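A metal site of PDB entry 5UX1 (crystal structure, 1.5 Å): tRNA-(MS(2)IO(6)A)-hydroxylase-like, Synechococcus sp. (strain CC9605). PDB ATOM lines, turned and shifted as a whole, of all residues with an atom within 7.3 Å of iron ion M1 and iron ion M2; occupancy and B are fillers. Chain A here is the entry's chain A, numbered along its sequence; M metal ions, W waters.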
ATOM      1  N   HIS A  49     -14.793 -16.752   8.047  1.00  0.00           N
ATOM      2  CA  HIS A  49     -15.778 -16.670   7.006  1.00  0.00           C
ATOM      3  C   HIS A  49     -16.910 -17.669   7.304  1.00  0.00           C
ATOM      4  O   HIS A  49     -18.090 -17.326   7.164  1.00  0.00           O
ATOM      5  CB  HIS A  49     -15.164 -16.945   5.647  1.00  0.00           C
ATOM      6  CG  HIS A  49     -16.147 -16.782   4.532  1.00  0.00           C
ATOM      7  ND1 HIS A  49     -16.978 -15.682   4.446  1.00  0.00           N
ATOM      8  CD2 HIS A  49     -16.483 -17.595   3.518  1.00  0.00           C
ATOM      9  CE1 HIS A  49     -17.761 -15.807   3.395  1.00  0.00           C
ATOM     10  NE2 HIS A  49     -17.481 -16.963   2.809  1.00  0.00           N
ATOM     11  N   CYS A  52     -19.013 -16.110   9.786  1.00  0.00           N
ATOM     12  CA  CYS A  52     -19.762 -14.975   9.201  1.00  0.00           C
ATOM     13  C   CYS A  52     -21.005 -15.463   8.464  1.00  0.00           C
ATOM     14  O   CYS A  52     -22.076 -14.818   8.579  1.00  0.00           O
ATOM     15  CB  CYS A  52     -18.893 -14.182   8.225  1.00  0.00           C
ATOM     16  SG  CYS A  52     -17.618 -13.143   9.018  1.00  0.00           S
ATOM     17  N   GLU A  53     -20.890 -16.578   7.730  1.00  0.00           N
ATOM     18  CA  GLU A  53     -22.041 -17.116   6.995  1.00  0.00           C
ATOM     19  C   GLU A  53     -23.098 -17.548   7.986  1.00  0.00           C
ATOM     20  O   GLU A  53     -24.295 -17.269   7.816  1.00  0.00           O
ATOM     21  CB  GLU A  53     -21.655 -18.278   6.072  1.00  0.00           C
ATOM     22  CG  GLU A  53     -20.560 -17.975   5.055  1.00  0.00           C
ATOM     23  CD  GLU A  53     -20.993 -17.402   3.704  1.00  0.00           C
ATOM     24  OE1 GLU A  53     -22.105 -16.862   3.561  1.00  0.00           O
ATOM     25  OE2 GLU A  53     -20.171 -17.502   2.753  1.00  0.00           O
ATOM     26  N   ALA A  56     -24.792 -14.548   9.494  1.00  0.00           N
ATOM     27  CA  ALA A  56     -25.711 -13.927   8.519  1.00  0.00           C
ATOM     28  C   ALA A  56     -27.048 -14.686   8.495  1.00  0.00           C
ATOM     29  O   ALA A  56     -28.149 -14.090   8.434  1.00  0.00           O
ATOM     30  CB  ALA A  56     -25.120 -13.860   7.160  1.00  0.00           C
ATOM     31  N   LEU A  80     -32.770 -16.816   1.911  1.00  0.00           N
ATOM     32  CA  LEU A  80     -31.456 -16.207   2.170  1.00  0.00           C
ATOM     33  C   LEU A  80     -30.776 -16.955   3.308  1.00  0.00           C
ATOM     34  O   LEU A  80     -29.618 -17.368   3.159  1.00  0.00           O
ATOM     35  CB  LEU A  80     -31.582 -14.698   2.493  1.00  0.00           C
ATOM     36  CG  LEU A  80     -30.272 -13.973   2.870  1.00  0.00           C
ATOM     37  CD1 LEU A  80     -30.337 -12.482   2.539  1.00  0.00           C
ATOM     38  CD2 LEU A  80     -29.903 -14.131   4.324  1.00  0.00           C
ATOM     39  N   GLU A  83     -29.482 -20.248   2.187  1.00  0.00           N
ATOM     40  CA  GLU A  83     -28.310 -20.134   1.366  1.00  0.00           C
ATOM     41  C   GLU A  83     -27.065 -19.816   2.198  1.00  0.00           C
ATOM     42  O   GLU A  83     -25.979 -20.377   1.934  1.00  0.00           O
ATOM     43  CB  GLU A  83     -28.541 -19.080   0.267  1.00  0.00           C
ATOM     44  CG  GLU A  83     -27.472 -19.086  -0.807  1.00  0.00           C
ATOM     45  CD  GLU A  83     -27.867 -18.320  -2.060  1.00  0.00           C
ATOM     46  OE1 GLU A  83     -28.741 -17.421  -1.972  1.00  0.00           O
ATOM     47  OE2 GLU A  83     -27.308 -18.642  -3.111  1.00  0.00           O
ATOM     48  N   GLU A  84     -27.210 -18.971   3.219  1.00  0.00           N
ATOM     49  CA  GLU A  84     -26.084 -18.709   4.110  1.00  0.00           C
ATOM     50  C   GLU A  84     -25.634 -19.966   4.875  1.00  0.00           C
ATOM     51  O   GLU A  84     -24.442 -20.161   5.088  1.00  0.00           O
ATOM     52  CB  GLU A  84     -26.379 -17.576   5.073  1.00  0.00           C
ATOM     53  CG  GLU A  84     -26.690 -16.214   4.390  1.00  0.00           C
ATOM     54  CD  GLU A  84     -25.622 -15.713   3.421  1.00  0.00           C
ATOM     55  OE1 GLU A  84     -24.880 -16.524   2.836  1.00  0.00           O
ATOM     56  OE2 GLU A  84     -25.554 -14.493   3.168  1.00  0.00           O
ATOM     57  N   LEU A  85     -26.591 -20.781   5.308  1.00  0.00           N
ATOM     58  CA  LEU A  85     -26.253 -22.055   5.934  1.00  0.00           C
ATOM     59  C   LEU A  85     -25.570 -23.018   4.964  1.00  0.00           C
ATOM     60  O   LEU A  85     -24.628 -23.719   5.353  1.00  0.00           O
ATOM     61  CB  LEU A  85     -27.465 -22.683   6.578  1.00  0.00           C
ATOM     62  CG  LEU A  85     -27.916 -21.934   7.855  1.00  0.00           C
ATOM     63  CD1 LEU A  85     -29.198 -22.557   8.386  1.00  0.00           C
ATOM     64  CD2 LEU A  85     -26.869 -21.851   8.973  1.00  0.00           C
ATOM     65  N   GLU A  86     -26.024 -23.046   3.697  1.00  0.00           N
ATOM     66  CA  GLU A  86     -25.332 -23.838   2.665  1.00  0.00           C
ATOM     67  C   GLU A  86     -23.895 -23.379   2.539  1.00  0.00           C
ATOM     68  O   GLU A  86     -22.974 -24.187   2.477  1.00  0.00           O
ATOM     69  CB  GLU A  86     -26.046 -23.736   1.329  1.00  0.00           C
ATOM     70  CG  GLU A  86     -27.405 -24.392   1.289  1.00  0.00           C
ATOM     71  CD  GLU A  86     -28.171 -24.168  -0.002  1.00  0.00           C
ATOM     72  OE1 GLU A  86     -27.671 -23.493  -0.911  1.00  0.00           O
ATOM     73  OE2 GLU A  86     -29.306 -24.671  -0.070  1.00  0.00           O
ATOM     74  N   HIS A  87     -23.673 -22.066   2.528  1.00  0.00           N
ATOM     75  CA  HIS A  87     -22.300 -21.562   2.448  1.00  0.00           C
ATOM     76  C   HIS A  87     -21.490 -21.956   3.683  1.00  0.00           C
ATOM     77  O   HIS A  87     -20.307 -22.375   3.567  1.00  0.00           O
ATOM     78  CB  HIS A  87     -22.320 -20.055   2.273  1.00  0.00           C
ATOM     79  CG  HIS A  87     -22.919 -19.637   0.978  1.00  0.00           C
ATOM     80  ND1 HIS A  87     -23.258 -18.338   0.711  1.00  0.00           N
ATOM     81  CD2 HIS A  87     -23.242 -20.354  -0.121  1.00  0.00           C
ATOM     82  CE1 HIS A  87     -23.768 -18.254  -0.502  1.00  0.00           C
ATOM     83  NE2 HIS A  87     -23.764 -19.469  -1.033  1.00  0.00           N
ATOM     84  N   PHE A  88     -22.101 -21.853   4.876  1.00  0.00           N
ATOM     85  CA  PHE A  88     -21.433 -22.282   6.090  1.00  0.00           C
ATOM     86  C   PHE A  88     -20.950 -23.722   5.937  1.00  0.00           C
ATOM     87  O   PHE A  88     -19.800 -24.027   6.271  1.00  0.00           O
ATOM     88  CB  PHE A  88     -22.374 -22.190   7.295  1.00  0.00           C
ATOM     89  CG  PHE A  88     -21.910 -22.958   8.486  1.00  0.00           C
ATOM     90  CD1 PHE A  88     -20.829 -22.532   9.238  1.00  0.00           C
ATOM     91  CD2 PHE A  88     -22.576 -24.110   8.889  1.00  0.00           C
ATOM     92  CE1 PHE A  88     -20.406 -23.241  10.331  1.00  0.00           C
ATOM     93  CE2 PHE A  88     -22.132 -24.829   9.988  1.00  0.00           C
ATOM     94  CZ  PHE A  88     -21.052 -24.399  10.703  1.00  0.00           C
ATOM     95  N   GLU A 137     -22.738  -7.683   3.870  1.00  0.00           N
ATOM     96  CA  GLU A 137     -22.682  -8.516   2.643  1.00  0.00           C
ATOM     97  C   GLU A 137     -21.848  -7.894   1.501  1.00  0.00           C
ATOM     98  O   GLU A 137     -21.068  -8.594   0.824  1.00  0.00           O
ATOM     99  CB  GLU A 137     -24.081  -8.830   2.097  1.00  0.00           C
ATOM    100  CG  GLU A 137     -24.988  -9.547   3.064  1.00  0.00           C
ATOM    101  CD  GLU A 137     -24.575 -10.989   3.272  1.00  0.00           C
ATOM    102  OE1 GLU A 137     -25.002 -11.838   2.461  1.00  0.00           O
ATOM    103  OE2 GLU A 137     -23.783 -11.247   4.224  1.00  0.00           O
ATOM    104  N   SER A 140     -18.203  -8.149   2.398  1.00  0.00           N
ATOM    105  CA  SER A 140     -17.760  -9.552   2.186  1.00  0.00           C
ATOM    106  C   SER A 140     -17.554  -9.832   0.704  1.00  0.00           C
ATOM    107  O   SER A 140     -16.531 -10.427   0.312  1.00  0.00           O
ATOM    108  CB  SER A 140     -18.764 -10.520   2.800  1.00  0.00           C
ATOM    109  OG  SER A 140     -18.790 -10.392   4.185  1.00  0.00           O
ATOM    110  N   MET A 144     -14.101 -10.911  -0.940  1.00  0.00           N
ATOM    111  CA  MET A 144     -14.057 -12.188  -1.648  1.00  0.00           C
ATOM    112  C   MET A 144     -13.653 -11.996  -3.087  1.00  0.00           C
ATOM    113  O   MET A 144     -12.912 -12.832  -3.646  1.00  0.00           O
ATOM    114  CB  MET A 144     -15.384 -12.916  -1.564  1.00  0.00           C
ATOM    115  CG  MET A 144     -15.661 -13.425  -0.169  1.00  0.00           C
ATOM    116  SD  MET A 144     -17.028 -14.603  -0.208  1.00  0.00           S
ATOM    117  CE  MET A 144     -18.333 -13.429  -0.252  1.00  0.00           C
ATOM    118  N   LEU A 163     -18.546 -18.143  -4.809  1.00  0.00           N
ATOM    119  CA  LEU A 163     -19.459 -17.469  -3.881  1.00  0.00           C
ATOM    120  C   LEU A 163     -19.914 -16.070  -4.292  1.00  0.00           C
ATOM    121  O   LEU A 163     -20.879 -15.541  -3.708  1.00  0.00           O
ATOM    122  CB  LEU A 163     -18.814 -17.417  -2.481  1.00  0.00           C
ATOM    123  CG  LEU A 163     -18.652 -18.776  -1.804  1.00  0.00           C
ATOM    124  CD1 LEU A 163     -17.729 -18.709  -0.597  1.00  0.00           C
ATOM    125  CD2 LEU A 163     -20.014 -19.342  -1.386  1.00  0.00           C
ATOM    126  N   SER A 166     -23.771 -15.155  -5.499  1.00  0.00           N
ATOM    127  CA  SER A 166     -24.785 -15.251  -4.459  1.00  0.00           C
ATOM    128  C   SER A 166     -24.689 -14.099  -3.489  1.00  0.00           C
ATOM    129  O   SER A 166     -25.722 -13.599  -3.041  1.00  0.00           O
ATOM    130  CB  SER A 166     -24.694 -16.585  -3.717  1.00  0.00           C
ATOM    131  OG  SER A 166     -23.393 -16.761  -3.197  1.00  0.00           O
ATOM    132  N   GLU A 167     -23.472 -13.667  -3.153  1.00  0.00           N
ATOM    133  CA  GLU A 167     -23.310 -12.526  -2.236  1.00  0.00           C
ATOM    134  C   GLU A 167     -23.898 -11.229  -2.840  1.00  0.00           C
ATOM    135  O   GLU A 167     -24.508 -10.425  -2.144  1.00  0.00           O
ATOM    136  CB  GLU A 167     -21.826 -12.332  -1.878  1.00  0.00           C
ATOM    137  CG  GLU A 167     -21.579 -11.853  -0.455  1.00  0.00           C
ATOM    138  CD  GLU A 167     -22.029 -12.876   0.581  1.00  0.00           C
ATOM    139  OE1 GLU A 167     -21.283 -13.847   0.876  1.00  0.00           O
ATOM    140  OE2 GLU A 167     -23.157 -12.695   1.095  1.00  0.00           O
ATOM    141  N   ALA A 168     -23.700 -11.034  -4.137  1.00  0.00           N
ATOM    142  CA  ALA A 168     -24.291  -9.907  -4.834  1.00  0.00           C
ATOM    143  C   ALA A 168     -25.817  -9.959  -4.840  1.00  0.00           C
ATOM    144  O   ALA A 168     -26.493  -8.925  -4.691  1.00  0.00           O
ATOM    145  CB  ALA A 168     -23.780  -9.822  -6.264  1.00  0.00           C
ATOM    146  N   ARG A 169     -26.383 -11.146  -4.992  1.00  0.00           N
ATOM    147  CA  ARG A 169     -27.852 -11.285  -4.860  1.00  0.00           C
ATOM    148  C   ARG A 169     -28.316 -10.906  -3.427  1.00  0.00           C
ATOM    149  O   ARG A 169     -29.399 -10.340  -3.231  1.00  0.00           O
ATOM    150  CB  ARG A 169     -28.324 -12.693  -5.272  1.00  0.00           C
ATOM    151  CG  ARG A 169     -28.162 -13.001  -6.756  1.00  0.00           C
ATOM    152  CD  ARG A 169     -28.890 -14.287  -7.148  1.00  0.00           C
ATOM    153  NE  ARG A 169     -28.283 -15.459  -6.504  1.00  0.00           N
ATOM    154  CZ  ARG A 169     -27.337 -16.242  -7.032  1.00  0.00           C
ATOM    155  NH1 ARG A 169     -26.838 -16.022  -8.244  1.00  0.00           N
ATOM    156  NH2 ARG A 169     -26.885 -17.273  -6.315  1.00  0.00           N
ATOM    157  N   HIS A 170     -27.484 -11.167  -2.424  1.00  0.00           N
ATOM    158  CA  HIS A 170     -27.881 -10.902  -1.054  1.00  0.00           C
ATOM    159  C   HIS A 170     -27.888  -9.416  -0.703  1.00  0.00           C
ATOM    160  O   HIS A 170     -28.848  -8.957  -0.084  1.00  0.00           O
ATOM    161  CB  HIS A 170     -26.995 -11.663  -0.078  1.00  0.00           C
ATOM    162  CG  HIS A 170     -27.114 -13.147  -0.176  1.00  0.00           C
ATOM    163  ND1 HIS A 170     -26.216 -13.996   0.421  1.00  0.00           N
ATOM    164  CD2 HIS A 170     -28.029 -13.927  -0.790  1.00  0.00           C
ATOM    165  CE1 HIS A 170     -26.552 -15.243   0.169  1.00  0.00           C
ATOM    166  NE2 HIS A 170     -27.659 -15.235  -0.563  1.00  0.00           N
ATOM    167  N   PHE A 171     -26.876  -8.654  -1.098  1.00  0.00           N
ATOM    168  CA  PHE A 171     -26.979  -7.213  -0.847  1.00  0.00           C
ATOM    169  C   PHE A 171     -28.041  -6.620  -1.743  1.00  0.00           C
ATOM    170  O   PHE A 171     -28.747  -5.681  -1.347  1.00  0.00           O
ATOM    171  CB  PHE A 171     -25.620  -6.431  -0.823  1.00  0.00           C
ATOM    172  CG  PHE A 171     -24.802  -6.488  -2.087  1.00  0.00           C
ATOM    173  CD1 PHE A 171     -25.116  -5.709  -3.195  1.00  0.00           C
ATOM    174  CD2 PHE A 171     -23.624  -7.243  -2.112  1.00  0.00           C
ATOM    175  CE1 PHE A 171     -24.312  -5.707  -4.330  1.00  0.00           C
ATOM    176  CE2 PHE A 171     -22.815  -7.246  -3.240  1.00  0.00           C
ATOM    177  CZ  PHE A 171     -23.165  -6.490  -4.353  1.00  0.00           C
ATOM    178  N   TYR A 174     -31.356  -6.971   0.196  1.00  0.00           N
ATOM    179  CA  TYR A 174     -31.551  -6.068   1.302  1.00  0.00           C
ATOM    180  C   TYR A 174     -31.903  -4.686   0.782  1.00  0.00           C
ATOM    181  O   TYR A 174     -32.732  -3.988   1.408  1.00  0.00           O
ATOM    182  CB  TYR A 174     -30.328  -6.061   2.223  1.00  0.00           C
ATOM    183  CG  TYR A 174     -30.346  -7.238   3.195  1.00  0.00           C
ATOM    184  CD1 TYR A 174     -31.355  -7.336   4.162  1.00  0.00           C
ATOM    185  CD2 TYR A 174     -29.387  -8.230   3.153  1.00  0.00           C
ATOM    186  CE1 TYR A 174     -31.408  -8.397   5.053  1.00  0.00           C
ATOM    187  CE2 TYR A 174     -29.425  -9.289   4.063  1.00  0.00           C
ATOM    188  CZ  TYR A 174     -30.445  -9.362   4.999  1.00  0.00           C
ATOM    189  OH  TYR A 174     -30.534 -10.384   5.939  1.00  0.00           O
HETATM  190 FE    FE M   1     -24.530 -13.701   1.826  1.00  0.00          FE
HETATM  191 FE    FE M   2     -22.905 -16.513   1.867  1.00  0.00          FE
HETATM  192  O   HOH W   1     -22.885 -13.968   3.558  1.00  0.00           O
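Iron ion M2 is bound by OE1 of Glu 53 (1.9 Å), ND1 of His 87 (2.2 Å) and OE1 of Glu 84 (2.2 Å).
Of the 22 residues printed, 4 come within 4 Å of iron ion M2. Along chain A the residues within 4 Å of iron ion M2 span positions 53 to 167. The nearest printed residue that does not touch iron ion M2 is His 170 (4.2 Å).
Water W1 lies within hydrogen-bond range of OE2 of Glu 137 and OE1 of Glu 167.
Four residues have an atom within 4 Å of iron ion M1: Glu 84, Glu 137, Glu 167 and His 170.
Iron ion M1 is bound by OE2 of Glu 167 (1.9 Å). OE2 of Glu 84 is bound to iron ion M1 (1.9 Å). OE1 of Glu 137 is bound to iron ion M1 (2.0 Å). ND1 of His 170 binds iron ion M1, 2.2 Å away. Iron ion M1 is bound by water W1. Iron ion M1 has five donor atoms within binding distance.
OE2 of Glu 53 lies within hydrogen-bond range of NE2 of His 49. A ring nitrogen (NE2) of His 87 lies close to the side-chain hydroxyl (OG) of Ser 166 (3.5 Å). A ring nitrogen (NE2) of His 170 sits at hydrogen-bond distance from the side-chain carboxylate of Glu 83.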
